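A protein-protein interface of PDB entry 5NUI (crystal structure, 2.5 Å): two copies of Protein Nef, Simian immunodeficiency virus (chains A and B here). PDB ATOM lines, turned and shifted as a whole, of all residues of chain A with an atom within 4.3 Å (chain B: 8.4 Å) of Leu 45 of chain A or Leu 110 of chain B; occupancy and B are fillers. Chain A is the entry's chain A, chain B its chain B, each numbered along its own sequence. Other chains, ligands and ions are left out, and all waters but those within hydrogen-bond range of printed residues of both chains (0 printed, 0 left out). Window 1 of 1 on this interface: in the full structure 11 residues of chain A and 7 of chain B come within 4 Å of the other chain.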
ATOM      1  N   ILE A  39      13.791   0.516   3.196  1.00  0.00           N
ATOM      2  CA  ILE A  39      14.433   1.832   3.130  1.00  0.00           C
ATOM      3  C   ILE A  39      15.951   1.699   3.207  1.00  0.00           C
ATOM      4  O   ILE A  39      16.694   2.340   2.444  1.00  0.00           O
ATOM      5  CB  ILE A  39      13.889   2.731   4.251  1.00  0.00           C
ATOM      6  CG1 ILE A  39      12.382   2.904   4.065  1.00  0.00           C
ATOM      7  CG2 ILE A  39      14.641   4.052   4.291  1.00  0.00           C
ATOM      8  CD1 ILE A  39      11.659   3.529   5.278  1.00  0.00           C
ATOM      9  N   GLY A  43      18.938   3.922  -0.819  1.00  0.00           N
ATOM     10  CA  GLY A  43      19.773   4.960  -0.242  1.00  0.00           C
ATOM     11  C   GLY A  43      19.359   5.154   1.182  1.00  0.00           C
ATOM     12  O   GLY A  43      20.170   5.257   2.056  1.00  0.00           O
ATOM     13  N   GLY A  44      18.078   5.172   1.413  1.00  0.00           N
ATOM     14  CA  GLY A  44      17.559   5.249   2.757  1.00  0.00           C
ATOM     15  C   GLY A  44      17.899   6.496   3.530  1.00  0.00           C
ATOM     16  O   GLY A  44      18.205   7.542   2.961  1.00  0.00           O
ATOM     17  N   LEU A  45      17.848   6.394   4.844  1.00  0.00           N
ATOM     18  CA  LEU A  45      17.973   7.548   5.721  1.00  0.00           C
ATOM     19  C   LEU A  45      19.374   7.708   6.274  1.00  0.00           C
ATOM     20  O   LEU A  45      19.654   8.705   6.953  1.00  0.00           O
ATOM     21  CB  LEU A  45      16.984   7.404   6.870  1.00  0.00           C
ATOM     22  CG  LEU A  45      15.568   7.188   6.343  1.00  0.00           C
ATOM     23  CD1 LEU A  45      14.795   6.222   7.211  1.00  0.00           C
ATOM     24  CD2 LEU A  45      14.860   8.565   6.257  1.00  0.00           C
ATOM     25  N   GLU A  46      20.238   6.723   6.016  1.00  0.00           N
ATOM     26  CA  GLU A  46      21.511   6.588   6.707  1.00  0.00           C
ATOM     27  C   GLU A  46      22.314   7.873   6.618  1.00  0.00           C
ATOM     28  O   GLU A  46      22.584   8.376   5.529  1.00  0.00           O
ATOM     29  CB  GLU A  46      22.300   5.415   6.109  1.00  0.00           C
ATOM     30  CG  GLU A  46      23.479   5.001   6.932  1.00  0.00           C
ATOM     31  CD  GLU A  46      23.115   4.577   8.334  1.00  0.00           C
ATOM     32  OE1 GLU A  46      23.962   4.759   9.228  1.00  0.00           O
ATOM     33  OE2 GLU A  46      22.007   4.052   8.560  1.00  0.00           O
ATOM     34  N   GLY A  47      22.673   8.407   7.780  1.00  0.00           N
ATOM     35  CA  GLY A  47      23.529   9.573   7.857  1.00  0.00           C
ATOM     36  C   GLY A  47      22.889  10.886   7.472  1.00  0.00           C
ATOM     37  O   GLY A  47      23.575  11.913   7.481  1.00  0.00           O
ATOM     38  N   ILE A  48      21.610  10.897   7.132  1.00  0.00           N
ATOM     39  CA  ILE A  48      20.966  12.108   6.649  1.00  0.00           C
ATOM     40  C   ILE A  48      20.509  12.963   7.819  1.00  0.00           C
ATOM     41  O   ILE A  48      19.994  12.460   8.837  1.00  0.00           O
ATOM     42  CB  ILE A  48      19.813  11.763   5.693  1.00  0.00           C
ATOM     43  CG1 ILE A  48      20.404  11.158   4.415  1.00  0.00           C
ATOM     44  CG2 ILE A  48      18.925  12.992   5.414  1.00  0.00           C
ATOM     45  CD1 ILE A  48      19.380  10.500   3.550  1.00  0.00           C
ATOM     46  N   ARG A  54      11.708  16.824   7.386  1.00  0.00           N
ATOM     47  CA  ARG A  54      12.011  15.507   6.835  1.00  0.00           C
ATOM     48  C   ARG A  54      11.275  14.405   7.584  1.00  0.00           C
ATOM     49  O   ARG A  54      10.950  13.367   6.994  1.00  0.00           O
ATOM     50  CB  ARG A  54      13.518  15.261   6.851  1.00  0.00           C
ATOM     51  CG  ARG A  54      14.231  15.830   5.633  1.00  0.00           C
ATOM     52  CD  ARG A  54      15.733  15.923   5.841  1.00  0.00           C
ATOM     53  NE  ARG A  54      16.364  16.724   4.797  1.00  0.00           N
ATOM     54  CZ  ARG A  54      17.648  17.065   4.789  1.00  0.00           C
ATOM     55  NH1 ARG A  54      18.449  16.664   5.776  1.00  0.00           N
ATOM     56  NH2 ARG A  54      18.127  17.818   3.803  1.00  0.00           N
ATOM     57  N   ILE A  57       7.894  14.360   5.886  1.00  0.00           N
ATOM     58  CA  ILE A  57       8.011  13.834   4.529  1.00  0.00           C
ATOM     59  C   ILE A  57       8.012  12.321   4.569  1.00  0.00           C
ATOM     60  O   ILE A  57       7.269  11.658   3.830  1.00  0.00           O
ATOM     61  CB  ILE A  57       9.275  14.378   3.841  1.00  0.00           C
ATOM     62  CG1 ILE A  57       9.165  15.885   3.609  1.00  0.00           C
ATOM     63  CG2 ILE A  57       9.544  13.608   2.545  1.00  0.00           C
ATOM     64  CD1 ILE A  57      10.419  16.498   3.057  1.00  0.00           C
ATOM     65  N   LEU A  58       8.827  11.754   5.461  1.00  0.00           N
ATOM     66  CA  LEU A  58       8.846  10.311   5.637  1.00  0.00           C
ATOM     67  C   LEU A  58       7.458   9.800   6.016  1.00  0.00           C
ATOM     68  O   LEU A  58       6.985   8.804   5.460  1.00  0.00           O
ATOM     69  CB  LEU A  58       9.901   9.941   6.690  1.00  0.00           C
ATOM     70  CG  LEU A  58       9.948   8.486   7.154  1.00  0.00           C
ATOM     71  CD1 LEU A  58      10.058   7.621   5.935  1.00  0.00           C
ATOM     72  CD2 LEU A  58      11.162   8.215   8.068  1.00  0.00           C
ATOM     73  N   TRP A  91      15.305   2.470  13.137  1.00  0.00           N
ATOM     74  CA  TRP A  91      16.026   3.714  12.925  1.00  0.00           C
ATOM     75  C   TRP A  91      16.016   4.538  14.196  1.00  0.00           C
ATOM     76  O   TRP A  91      14.966   4.701  14.825  1.00  0.00           O
ATOM     77  CB  TRP A  91      15.420   4.507  11.784  1.00  0.00           C
ATOM     78  CG  TRP A  91      15.543   3.850  10.469  1.00  0.00           C
ATOM     79  CD1 TRP A  91      14.636   3.029   9.885  1.00  0.00           C
ATOM     80  CD2 TRP A  91      16.643   3.954   9.557  1.00  0.00           C
ATOM     81  NE1 TRP A  91      15.096   2.628   8.653  1.00  0.00           N
ATOM     82  CE2 TRP A  91      16.324   3.183   8.432  1.00  0.00           C
ATOM     83  CE3 TRP A  91      17.861   4.631   9.583  1.00  0.00           C
ATOM     84  CZ2 TRP A  91      17.179   3.056   7.352  1.00  0.00           C
ATOM     85  CZ3 TRP A  91      18.710   4.507   8.504  1.00  0.00           C
ATOM     86  CH2 TRP A  91      18.364   3.733   7.403  1.00  0.00           C
ATOM     87  N   TRP A 129      19.903  10.343  11.150  1.00  0.00           N
ATOM     88  CA  TRP A 129      19.285   9.029  11.147  1.00  0.00           C
ATOM     89  C   TRP A 129      20.372   7.952  11.107  1.00  0.00           C
ATOM     90  O   TRP A 129      21.333   8.048  10.332  1.00  0.00           O
ATOM     91  CB  TRP A 129      18.341   8.898   9.939  1.00  0.00           C
ATOM     92  CG  TRP A 129      16.855   9.183  10.210  1.00  0.00           C
ATOM     93  CD1 TRP A 129      15.994   8.417  10.937  1.00  0.00           C
ATOM     94  CD2 TRP A 129      16.060  10.269   9.681  1.00  0.00           C
ATOM     95  NE1 TRP A 129      14.730   8.977  10.935  1.00  0.00           N
ATOM     96  CE2 TRP A 129      14.747  10.108  10.167  1.00  0.00           C
ATOM     97  CE3 TRP A 129      16.339  11.362   8.864  1.00  0.00           C
ATOM     98  CZ2 TRP A 129      13.721  10.997   9.861  1.00  0.00           C
ATOM     99  CZ3 TRP A 129      15.310  12.243   8.562  1.00  0.00           C
ATOM    100  CH2 TRP A 129      14.021  12.055   9.062  1.00  0.00           C
ATOM    101  N   GLN B 103       7.792  18.774  -2.454  1.00  0.00           N
ATOM    102  CA  GLN B 103       9.146  18.285  -2.201  1.00  0.00           C
ATOM    103  C   GLN B 103       9.353  16.866  -2.714  1.00  0.00           C
ATOM    104  O   GLN B 103       9.511  15.937  -1.922  1.00  0.00           O
ATOM    105  CB  GLN B 103       9.467  18.325  -0.700  1.00  0.00           C
ATOM    106  N   GLU B 104       9.353  16.690  -4.036  1.00  0.00           N
ATOM    107  CA  GLU B 104       9.680  15.377  -4.580  1.00  0.00           C
ATOM    108  C   GLU B 104      11.183  15.161  -4.694  1.00  0.00           C
ATOM    109  O   GLU B 104      11.628  14.009  -4.754  1.00  0.00           O
ATOM    110  CB  GLU B 104       9.019  15.176  -5.947  1.00  0.00           C
ATOM    111  CG  GLU B 104       9.007  13.716  -6.422  1.00  0.00           C
ATOM    112  CD  GLU B 104       7.693  13.013  -6.144  1.00  0.00           C
ATOM    113  N   ASP B 105      11.975  16.231  -4.710  1.00  0.00           N
ATOM    114  CA  ASP B 105      13.422  16.054  -4.742  1.00  0.00           C
ATOM    115  C   ASP B 105      13.981  15.763  -3.353  1.00  0.00           C
ATOM    116  O   ASP B 105      14.886  14.937  -3.210  1.00  0.00           O
ATOM    117  CB  ASP B 105      14.095  17.286  -5.344  1.00  0.00           C
ATOM    118  CG  ASP B 105      15.383  16.943  -6.063  1.00  0.00           C
ATOM    119  OD1 ASP B 105      15.831  15.781  -5.952  1.00  0.00           O
ATOM    120  OD2 ASP B 105      15.941  17.824  -6.751  1.00  0.00           O
ATOM    121  N   GLU B 106      13.455  16.431  -2.324  1.00  0.00           N
ATOM    122  CA  GLU B 106      13.821  16.099  -0.955  1.00  0.00           C
ATOM    123  C   GLU B 106      13.316  14.718  -0.576  1.00  0.00           C
ATOM    124  O   GLU B 106      13.989  13.981   0.159  1.00  0.00           O
ATOM    125  CB  GLU B 106      13.264  17.148   0.003  1.00  0.00           C
ATOM    126  CG  GLU B 106      13.698  16.964   1.443  1.00  0.00           C
ATOM    127  CD  GLU B 106      13.768  18.278   2.194  1.00  0.00           C
ATOM    128  OE1 GLU B 106      14.789  18.516   2.889  1.00  0.00           O
ATOM    129  OE2 GLU B 106      12.801  19.066   2.084  1.00  0.00           O
ATOM    130  N   GLU B 107      12.134  14.357  -1.072  1.00  0.00           N
ATOM    131  CA  GLU B 107      11.629  13.006  -0.891  1.00  0.00           C
ATOM    132  C   GLU B 107      12.577  11.978  -1.492  1.00  0.00           C
ATOM    133  O   GLU B 107      12.777  10.897  -0.924  1.00  0.00           O
ATOM    134  CB  GLU B 107      10.246  12.904  -1.520  1.00  0.00           C
ATOM    135  CG  GLU B 107       9.688  11.520  -1.626  1.00  0.00           C
ATOM    136  CD  GLU B 107       8.232  11.565  -2.012  1.00  0.00           C
ATOM    137  OE1 GLU B 107       7.458  10.748  -1.469  1.00  0.00           O
ATOM    138  OE2 GLU B 107       7.864  12.436  -2.843  1.00  0.00           O
ATOM    139  N   HIS B 108      13.188  12.301  -2.630  1.00  0.00           N
ATOM    140  CA  HIS B 108      14.076  11.344  -3.280  1.00  0.00           C
ATOM    141  C   HIS B 108      15.375  11.183  -2.504  1.00  0.00           C
ATOM    142  O   HIS B 108      15.838  10.056  -2.286  1.00  0.00           O
ATOM    143  CB  HIS B 108      14.352  11.775  -4.717  1.00  0.00           C
ATOM    144  CG  HIS B 108      13.370  11.225  -5.700  1.00  0.00           C
ATOM    145  ND1 HIS B 108      12.086  11.709  -5.816  1.00  0.00           N
ATOM    146  CD2 HIS B 108      13.476  10.212  -6.592  1.00  0.00           C
ATOM    147  CE1 HIS B 108      11.444  11.027  -6.747  1.00  0.00           C
ATOM    148  NE2 HIS B 108      12.264  10.112  -7.232  1.00  0.00           N
ATOM    149  N   TYR B 109      15.978  12.297  -2.077  1.00  0.00           N
ATOM    150  CA  TYR B 109      17.211  12.217  -1.302  1.00  0.00           C
ATOM    151  C   TYR B 109      17.006  11.413  -0.023  1.00  0.00           C
ATOM    152  O   TYR B 109      17.872  10.619   0.384  1.00  0.00           O
ATOM    153  CB  TYR B 109      17.697  13.623  -0.987  1.00  0.00           C
ATOM    154  CG  TYR B 109      18.852  13.716  -0.019  1.00  0.00           C
ATOM    155  CD1 TYR B 109      20.148  13.410  -0.409  1.00  0.00           C
ATOM    156  CD2 TYR B 109      18.652  14.170   1.271  1.00  0.00           C
ATOM    157  CE1 TYR B 109      21.212  13.528   0.477  1.00  0.00           C
ATOM    158  CE2 TYR B 109      19.705  14.288   2.163  1.00  0.00           C
ATOM    159  CZ  TYR B 109      20.983  13.965   1.761  1.00  0.00           C
ATOM    160  OH  TYR B 109      22.030  14.081   2.652  1.00  0.00           O
ATOM    161  N   LEU B 110      15.882  11.641   0.596  1.00  0.00           N
ATOM    162  CA  LEU B 110      15.549  10.965   1.792  1.00  0.00           C
ATOM    163  C   LEU B 110      15.337   9.488   1.615  1.00  0.00           C
ATOM    164  O   LEU B 110      15.733   8.727   2.456  1.00  0.00           O
ATOM    165  CB  LEU B 110      14.301  11.587   2.347  1.00  0.00           C
ATOM    166  CG  LEU B 110      14.050  11.370   3.810  1.00  0.00           C
ATOM    167  CD1 LEU B 110      15.164  12.056   4.532  1.00  0.00           C
ATOM    168  CD2 LEU B 110      12.745  12.002   4.199  1.00  0.00           C
ATOM    169  N   MET B 111      14.690   9.079   0.540  1.00  0.00           N
ATOM    170  CA  MET B 111      14.386   7.670   0.373  1.00  0.00           C
ATOM    171  C   MET B 111      14.962   6.837  -0.738  1.00  0.00           C
ATOM    172  O   MET B 111      15.389   5.747  -0.497  1.00  0.00           O
ATOM    173  CB  MET B 111      12.892   7.495   0.296  1.00  0.00           C
ATOM    174  CG  MET B 111      12.089   8.489   1.092  1.00  0.00           C
ATOM    175  SD  MET B 111      11.848   7.961   2.763  1.00  0.00           S
ATOM    176  CE  MET B 111      11.612   6.228   2.507  1.00  0.00           C
ATOM    177  N   HIS B 112      14.921   7.313  -1.963  1.00  0.00           N
ATOM    178  CA  HIS B 112      15.407   6.533  -3.084  1.00  0.00           C
ATOM    179  C   HIS B 112      16.276   7.406  -3.922  1.00  0.00           C
ATOM    180  O   HIS B 112      15.875   7.891  -4.960  1.00  0.00           O
ATOM    181  CB  HIS B 112      14.242   6.030  -3.908  1.00  0.00           C
ATOM    182  CG  HIS B 112      14.664   5.191  -5.061  1.00  0.00           C
ATOM    183  ND1 HIS B 112      14.181   3.922  -5.273  1.00  0.00           N
ATOM    184  CD2 HIS B 112      15.560   5.424  -6.043  1.00  0.00           C
ATOM    185  CE1 HIS B 112      14.742   3.417  -6.353  1.00  0.00           C
ATOM    186  NE2 HIS B 112      15.584   4.308  -6.838  1.00  0.00           N
ATOM    187  N   PRO B 113      17.484   7.622  -3.462  1.00  0.00           N
ATOM    188  CA  PRO B 113      18.404   8.564  -4.135  1.00  0.00           C
ATOM    189  C   PRO B 113      18.768   8.203  -5.580  1.00  0.00           C
ATOM    190  O   PRO B 113      19.447   9.010  -6.229  1.00  0.00           O
ATOM    191  CB  PRO B 113      19.655   8.549  -3.241  1.00  0.00           C
ATOM    192  CG  PRO B 113      19.265   7.868  -1.975  1.00  0.00           C
ATOM    193  CD  PRO B 113      17.972   7.162  -2.151  1.00  0.00           C
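No position is printed for both chains. Of the 12 pairs that touch across the chains among the printed residues, none has its exchanged pair printed and touching as well.
N of Gly 44 of chain A is in hydrogen-bond range of O of Met 111 of chain B (3.3 Å). The side-chain carboxylate of Glu 106 of chain B lies within salt-bridge range of the guanidinium group of Arg 54 of chain A, 3.1 Å away. The backbone carbonyl oxygen of Gly 44 of chain A sits close to the backbone carbonyl oxygen of Leu 110 of chain B (2.8 Å).
Hydrophobic or aromatic side chains of chain A within 4 Å of the printed part of chain B: Ile 39, Leu 45, Ile 48, Ile 57 and Leu 58.
Leu 45 of chain A touches one residue of chain B. Of chain B, only Leu 110 (2.8 Å) and Met 111 (3.3 Å) come within 4 Å of Gly 44 of chain A. Of the printed residues of chain A, Met 111 of chain B touches Ile 39, Gly 44 and Leu 58. Of the printed residues of chain B, Ile 39 of chain A touches Met 111. Of the printed residues of chain A, Glu 106 of chain B touches Arg 54 and Ile 57. Trp 91 of chain A touches none of the printed residues of chain B.
The backbone carbonyl oxygen of Ile 39 of chain A sits close to the backbone NH of Gly 44 of chain A (3.3 Å). O of Ile 48 of chain A lies within hydrogen-bond range of N of Trp 129 of chain A, 3.1 Å away.
Ile 39 of chain A touches Met 111 of chain B. Gly 43 of chain A touches Pro 113 of chain B (CA to CG, 3.4 Å). Leu 45 of chain A touches Leu 110 of chain B (CD2 to CG, 3.8 Å). Ile 48 of chain A touches Tyr 109 of chain B (CD1 to O, 3.5 Å). Leu 110 of chain B touches Ile 48 of chain A (CD1 to CG2, 3.97 Å). Arg 54 of chain A touches Leu 110 of chain B. Glu 106 of chain B touches Ile 57 of chain A (OE2 to CD1, 3.6 Å). Ile 57 of chain A touches Leu 110 of chain B. CD1 of Leu 58 of chain A touches SD of Met 111 of chain B (3.7 Å).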
